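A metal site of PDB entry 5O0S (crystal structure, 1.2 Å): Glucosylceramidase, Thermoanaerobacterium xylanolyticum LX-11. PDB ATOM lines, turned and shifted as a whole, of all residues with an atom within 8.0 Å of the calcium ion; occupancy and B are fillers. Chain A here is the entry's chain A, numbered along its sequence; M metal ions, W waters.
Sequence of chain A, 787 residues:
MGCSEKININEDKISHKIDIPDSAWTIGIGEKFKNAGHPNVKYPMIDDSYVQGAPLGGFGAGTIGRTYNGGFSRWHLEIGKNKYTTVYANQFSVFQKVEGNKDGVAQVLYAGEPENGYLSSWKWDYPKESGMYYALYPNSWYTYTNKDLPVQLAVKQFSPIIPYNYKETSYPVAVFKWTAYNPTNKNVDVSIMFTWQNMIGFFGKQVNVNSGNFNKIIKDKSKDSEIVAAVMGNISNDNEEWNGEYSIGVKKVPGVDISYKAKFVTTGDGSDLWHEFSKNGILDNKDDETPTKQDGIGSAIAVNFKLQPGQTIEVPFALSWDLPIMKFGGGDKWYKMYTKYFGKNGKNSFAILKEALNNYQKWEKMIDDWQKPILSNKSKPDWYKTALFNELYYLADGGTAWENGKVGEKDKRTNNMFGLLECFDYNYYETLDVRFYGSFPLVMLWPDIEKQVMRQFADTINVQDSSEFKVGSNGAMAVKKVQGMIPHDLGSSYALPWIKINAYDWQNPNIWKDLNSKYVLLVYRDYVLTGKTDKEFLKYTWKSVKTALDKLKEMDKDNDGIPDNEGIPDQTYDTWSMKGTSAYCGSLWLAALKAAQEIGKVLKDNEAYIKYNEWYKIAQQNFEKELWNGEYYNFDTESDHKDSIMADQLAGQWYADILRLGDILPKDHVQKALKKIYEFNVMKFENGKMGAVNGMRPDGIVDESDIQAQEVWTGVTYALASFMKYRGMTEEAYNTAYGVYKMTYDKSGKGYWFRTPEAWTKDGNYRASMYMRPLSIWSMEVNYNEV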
ATOM      1  N   LYS A 553      -3.150  38.306   5.756  1.00  0.00           N
ATOM      2  CA  LYS A 553      -1.954  37.573   6.187  1.00  0.00           C
ATOM      3  C   LYS A 553      -2.027  37.118   7.651  1.00  0.00           C
ATOM      4  O   LYS A 553      -1.469  36.082   8.023  1.00  0.00           O
ATOM      5  CB  LYS A 553      -0.699  38.426   5.973  1.00  0.00           C
ATOM      6  CG  LYS A 553       0.620  37.748   6.358  1.00  0.00           C
ATOM      7  CD  LYS A 553       0.888  36.501   5.543  1.00  0.00           C
ATOM      8  CE  LYS A 553       2.327  36.252   5.203  1.00  0.00           C
ATOM      9  NZ  LYS A 553       3.224  36.202   6.346  1.00  0.00           N
ATOM     10  N   MET A 555      -4.381  35.844   9.050  1.00  0.00           N
ATOM     11  CA  MET A 555      -5.175  34.631   9.130  1.00  0.00           C
ATOM     12  C   MET A 555      -4.391  33.361   8.766  1.00  0.00           C
ATOM     13  O   MET A 555      -4.956  32.268   8.692  1.00  0.00           O
ATOM     14  CB  MET A 555      -6.404  34.787   8.285  1.00  0.00           C
ATOM     15  CG  MET A 555      -7.250  35.960   8.790  1.00  0.00           C
ATOM     16  SD  MET A 555      -8.620  36.262   7.737  1.00  0.00           S
ATOM     17  CE  MET A 555      -9.530  37.462   8.683  1.00  0.00           C
ATOM     18  N   ASP A 556      -3.092  33.506   8.550  1.00  0.00           N
ATOM     19  CA  ASP A 556      -2.208  32.370   8.325  1.00  0.00           C
ATOM     20  C   ASP A 556      -1.776  31.857   9.696  1.00  0.00           C
ATOM     21  O   ASP A 556      -0.797  32.336  10.234  1.00  0.00           O
ATOM     22  CB  ASP A 556      -0.978  32.826   7.548  1.00  0.00           C
ATOM     23  CG  ASP A 556       0.043  31.738   7.384  1.00  0.00           C
ATOM     24  OD1 ASP A 556      -0.316  30.548   7.494  1.00  0.00           O
ATOM     25  OD2 ASP A 556       1.209  32.065   7.159  1.00  0.00           O
ATOM     26  N   LYS A 557      -2.466  30.877  10.234  1.00  0.00           N
ATOM     27  CA  LYS A 557      -2.166  30.388  11.586  1.00  0.00           C
ATOM     28  C   LYS A 557      -1.081  29.315  11.651  1.00  0.00           C
ATOM     29  O   LYS A 557      -0.562  29.058  12.702  1.00  0.00           O
ATOM     30  CB  LYS A 557      -3.409  29.877  12.308  1.00  0.00           C
ATOM     31  CG  LYS A 557      -4.579  30.863  12.395  1.00  0.00           C
ATOM     32  CD  LYS A 557      -5.851  30.182  12.911  1.00  0.00           C
ATOM     33  CE  LYS A 557      -6.840  31.141  13.583  1.00  0.00           C
ATOM     34  NZ  LYS A 557      -7.910  31.657  12.679  1.00  0.00           N
ATOM     35  N   ASP A 558      -0.751  28.676  10.531  1.00  0.00           N
ATOM     36  CA  ASP A 558       0.291  27.641  10.595  1.00  0.00           C
ATOM     37  C   ASP A 558       1.613  28.103   9.977  1.00  0.00           C
ATOM     38  O   ASP A 558       2.555  27.311   9.845  1.00  0.00           O
ATOM     39  CB  ASP A 558      -0.173  26.329   9.982  1.00  0.00           C
ATOM     40  CG  ASP A 558      -0.363  26.413   8.503  1.00  0.00           C
ATOM     41  OD1 ASP A 558      -0.605  27.535   8.012  1.00  0.00           O
ATOM     42  OD2 ASP A 558      -0.258  25.363   7.833  1.00  0.00           O
ATOM     43  N   ASN A 559       1.684  29.389   9.633  1.00  0.00           N
ATOM     44  CA  ASN A 559       2.891  29.999   9.107  1.00  0.00           C
ATOM     45  C   ASN A 559       3.425  29.367   7.799  1.00  0.00           C
ATOM     46  O   ASN A 559       4.622  29.363   7.573  1.00  0.00           O
ATOM     47  CB  ASN A 559       3.983  30.058  10.189  1.00  0.00           C
ATOM     48  CG  ASN A 559       4.973  31.172   9.938  1.00  0.00           C
ATOM     49  OD1 ASN A 559       4.591  32.298   9.586  1.00  0.00           O
ATOM     50  ND2 ASN A 559       6.250  30.864  10.075  1.00  0.00           N
ATOM     51  N   ASP A 560       2.521  28.881   6.932  1.00  0.00           N
ATOM     52  CA  ASP A 560       2.906  28.444   5.554  1.00  0.00           C
ATOM     53  C   ASP A 560       2.847  29.599   4.547  1.00  0.00           C
ATOM     54  O   ASP A 560       3.085  29.408   3.359  1.00  0.00           O
ATOM     55  CB  ASP A 560       2.124  27.218   5.072  1.00  0.00           C
ATOM     56  CG  ASP A 560       0.720  27.526   4.664  1.00  0.00           C
ATOM     57  OD1 ASP A 560       0.197  28.626   4.983  1.00  0.00           O
ATOM     58  OD2 ASP A 560       0.068  26.637   4.081  1.00  0.00           O
ATOM     59  N   GLY A 561       2.516  30.797   5.020  1.00  0.00           N
ATOM     60  CA  GLY A 561       2.447  31.967   4.171  1.00  0.00           C
ATOM     61  C   GLY A 561       1.100  32.236   3.512  1.00  0.00           C
ATOM     62  O   GLY A 561       0.975  33.194   2.770  1.00  0.00           O
ATOM     63  N   ILE A 562       0.122  31.397   3.813  1.00  0.00           N
ATOM     64  CA  ILE A 562      -1.168  31.434   3.111  1.00  0.00           C
ATOM     65  C   ILE A 562      -2.268  31.528   4.176  1.00  0.00           C
ATOM     66  O   ILE A 562      -2.219  30.792   5.158  1.00  0.00           O
ATOM     67  CB  ILE A 562      -1.405  30.134   2.301  1.00  0.00           C
ATOM     68  CG1 ILE A 562      -0.255  29.897   1.317  1.00  0.00           C
ATOM     69  CG2 ILE A 562      -2.729  30.190   1.528  1.00  0.00           C
ATOM     70  CD1 ILE A 562      -0.216  28.512   0.742  1.00  0.00           C
ATOM     71  N   PRO A 563      -3.289  32.407   4.033  1.00  0.00           N
ATOM     72  CA  PRO A 563      -4.394  32.364   4.988  1.00  0.00           C
ATOM     73  C   PRO A 563      -5.043  30.963   5.072  1.00  0.00           C
ATOM     74  O   PRO A 563      -5.174  30.303   4.059  1.00  0.00           O
ATOM     75  CB  PRO A 563      -5.397  33.374   4.426  1.00  0.00           C
ATOM     76  CG  PRO A 563      -5.012  33.533   2.987  1.00  0.00           C
ATOM     77  CD  PRO A 563      -3.540  33.362   2.937  1.00  0.00           C
ATOM     78  N   ASP A 564      -5.463  30.555   6.268  1.00  0.00           N
ATOM     79  CA  ASP A 564      -6.034  29.222   6.515  1.00  0.00           C
ATOM     80  C   ASP A 564      -7.535  29.295   6.497  1.00  0.00           C
ATOM     81  O   ASP A 564      -8.135  29.996   7.326  1.00  0.00           O
ATOM     82  CB  ASP A 564      -5.641  28.654   7.885  1.00  0.00           C
ATOM     83  CG  ASP A 564      -4.270  28.087   7.922  1.00  0.00           C
ATOM     84  OD1 ASP A 564      -3.347  28.924   7.996  1.00  0.00           O
ATOM     85  OD2 ASP A 564      -4.117  26.824   7.914  1.00  0.00           O
ATOM     86  N   ASN A 565      -8.173  28.505   5.634  1.00  0.00           N
ATOM     87  CA  ASN A 565      -9.586  28.337   5.734  1.00  0.00           C
ATOM     88  C   ASN A 565      -9.864  27.566   7.031  1.00  0.00           C
ATOM     89  O   ASN A 565      -9.086  26.680   7.435  1.00  0.00           O
ATOM     90  CB  ASN A 565     -10.164  27.613   4.506  1.00  0.00           C
ATOM     91  CG  ASN A 565     -10.096  28.452   3.249  1.00  0.00           C
ATOM     92  OD1 ASN A 565      -9.201  28.302   2.427  1.00  0.00           O
ATOM     93  ND2 ASN A 565     -11.068  29.321   3.078  1.00  0.00           N
ATOM     94  N   GLY A 580      -7.710  24.476   6.008  1.00  0.00           N
ATOM     95  CA  GLY A 580      -6.292  24.487   5.766  1.00  0.00           C
ATOM     96  C   GLY A 580      -6.014  25.397   4.600  1.00  0.00           C
ATOM     97  O   GLY A 580      -6.630  26.434   4.454  1.00  0.00           O
ATOM     98  N   THR A 581      -5.092  24.997   3.737  1.00  0.00           N
ATOM     99  CA  THR A 581      -4.918  25.729   2.494  1.00  0.00           C
ATOM    100  C   THR A 581      -5.856  25.176   1.453  1.00  0.00           C
ATOM    101  O   THR A 581      -5.871  23.990   1.236  1.00  0.00           O
ATOM    102  CB  THR A 581      -3.466  25.604   1.994  1.00  0.00           C
ATOM    103  OG1 THR A 581      -2.588  26.278   2.915  1.00  0.00           O
ATOM    104  CG2 THR A 581      -3.310  26.248   0.642  1.00  0.00           C
ATOM    105  N   TRP A 589      -5.104  34.265  -3.331  1.00  0.00           N
ATOM    106  CA  TRP A 589      -4.051  34.926  -2.520  1.00  0.00           C
ATOM    107  C   TRP A 589      -2.755  35.089  -3.286  1.00  0.00           C
ATOM    108  O   TRP A 589      -2.204  36.190  -3.319  1.00  0.00           O
ATOM    109  CB  TRP A 589      -3.864  34.093  -1.251  1.00  0.00           C
ATOM    110  CG  TRP A 589      -2.688  34.469  -0.368  1.00  0.00           C
ATOM    111  CD1 TRP A 589      -1.602  33.716  -0.104  1.00  0.00           C
ATOM    112  CD2 TRP A 589      -2.528  35.682   0.400  1.00  0.00           C
ATOM    113  NE1 TRP A 589      -0.762  34.375   0.768  1.00  0.00           N
ATOM    114  CE2 TRP A 589      -1.332  35.571   1.121  1.00  0.00           C
ATOM    115  CE3 TRP A 589      -3.337  36.806   0.618  1.00  0.00           C
ATOM    116  CZ2 TRP A 589      -0.865  36.571   1.994  1.00  0.00           C
ATOM    117  CZ3 TRP A 589      -2.857  37.841   1.472  1.00  0.00           C
ATOM    118  CH2 TRP A 589      -1.639  37.705   2.155  1.00  0.00           C
ATOM    119  N   ASN A 622       4.840  26.777  -1.055  1.00  0.00           N
ATOM    120  CA  ASN A 622       4.016  25.935  -0.193  1.00  0.00           C
ATOM    121  C   ASN A 622       2.685  25.515  -0.825  1.00  0.00           C
ATOM    122  O   ASN A 622       2.244  24.373  -0.611  1.00  0.00           O
ATOM    123  CB  ASN A 622       3.805  26.599   1.179  1.00  0.00           C
ATOM    124  CG  ASN A 622       5.033  26.596   1.988  1.00  0.00           C
ATOM    125  OD1 ASN A 622       5.879  25.716   1.810  1.00  0.00           O
ATOM    126  ND2 ASN A 622       5.220  27.601   2.824  1.00  0.00           N
ATOM    127  N   GLU A 626       1.768  21.640  -1.072  1.00  0.00           N
ATOM    128  CA  GLU A 626       0.607  21.175  -0.318  1.00  0.00           C
ATOM    129  C   GLU A 626      -0.499  20.584  -1.178  1.00  0.00           C
ATOM    130  O   GLU A 626      -1.190  19.675  -0.734  1.00  0.00           O
ATOM    131  CB  GLU A 626       0.014  22.333   0.492  1.00  0.00           C
ATOM    132  CG  GLU A 626       0.866  22.768   1.693  1.00  0.00           C
ATOM    133  CD  GLU A 626       0.423  24.094   2.282  1.00  0.00           C
ATOM    134  OE1 GLU A 626      -0.628  24.620   1.940  1.00  0.00           O
ATOM    135  OE2 GLU A 626       1.190  24.638   3.107  1.00  0.00           O
ATOM    136  N   THR A 637      -6.262  21.090   2.079  1.00  0.00           N
ATOM    137  CA  THR A 637      -5.300  20.229   2.766  1.00  0.00           C
ATOM    138  C   THR A 637      -5.874  19.408   3.934  1.00  0.00           C
ATOM    139  O   THR A 637      -5.226  18.433   4.343  1.00  0.00           O
ATOM    140  CB  THR A 637      -4.112  21.026   3.300  1.00  0.00           C
ATOM    141  OG1 THR A 637      -4.563  22.106   4.141  1.00  0.00           O
ATOM    142  CG2 THR A 637      -3.279  21.588   2.191  1.00  0.00           C
ATOM    143  N   GLU A 638      -7.031  19.785   4.472  1.00  0.00           N
ATOM    144  CA  GLU A 638      -7.540  19.183   5.740  1.00  0.00           C
ATOM    145  C   GLU A 638      -8.963  18.613   5.737  1.00  0.00           C
ATOM    146  O   GLU A 638      -9.326  17.928   6.699  1.00  0.00           O
ATOM    147  CB  GLU A 638      -7.432  20.200   6.874  1.00  0.00           C
ATOM    148  CG  GLU A 638      -6.000  20.613   7.162  1.00  0.00           C
ATOM    149  CD  GLU A 638      -5.821  21.576   8.315  1.00  0.00           C
ATOM    150  OE1 GLU A 638      -6.609  21.546   9.283  1.00  0.00           O
ATOM    151  OE2 GLU A 638      -4.850  22.352   8.296  1.00  0.00           O
HETATM  152 CA    CA M   1      -1.633  28.939   6.374  1.00  0.00          CA
HETATM  153  O   HOH W   1      -3.251  27.801   4.744  1.00  0.00           O
HETATM  154  O   HOH W   2      -2.138  26.301   6.199  1.00  0.00           O
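OE2 of Glu 626 sits close to OD2 of Asp 560, at 2.5 Å. The backbone NH (N) of Asp 564 sits at hydrogen-bond distance from the backbone carbonyl oxygen (O) of Met 555 (3.0 Å). OD1 of Asp 556 sits close to N of Asn 559, at 3.1 Å. The side-chain carboxylate of Asp 560 sits at hydrogen-bond distance from the side-chain hydroxyl of Thr 581 (2.9 Å). The backbone carbonyl oxygen (O) of Asp 560 sits at hydrogen-bond distance from the side-chain amide nitrogen (ND2) of Asn 622 (2.8 Å). The side-chain carboxylate of Asp 556 lies within hydrogen-bond range of the backbone NH of Gly 561, 2.8 Å away. N of Lys 557 sits close to OD1 of Asp 564 (3.1 Å).
Along chain A the residues within 4 Å of the calcium ion span positions 556 to 564.
The calcium ion is bound by the backbone carbonyl oxygen of Ile 562 (2.3 Å), the side-chain carboxylate of Asp 560 (2.3 Å), the side-chain carboxylate of Asp 564 (2.4 Å), the side-chain carboxylate of Asp 556 (2.4 Å), the side-chain carboxylate of Asp 558 (2.4 Å), water W1 (2.6 Å) and water W2 (2.7 Å).
Water W1 lies within hydrogen-bond range of OG1 of Thr 581, O of Pro 563 and OD2 of Asp 564.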
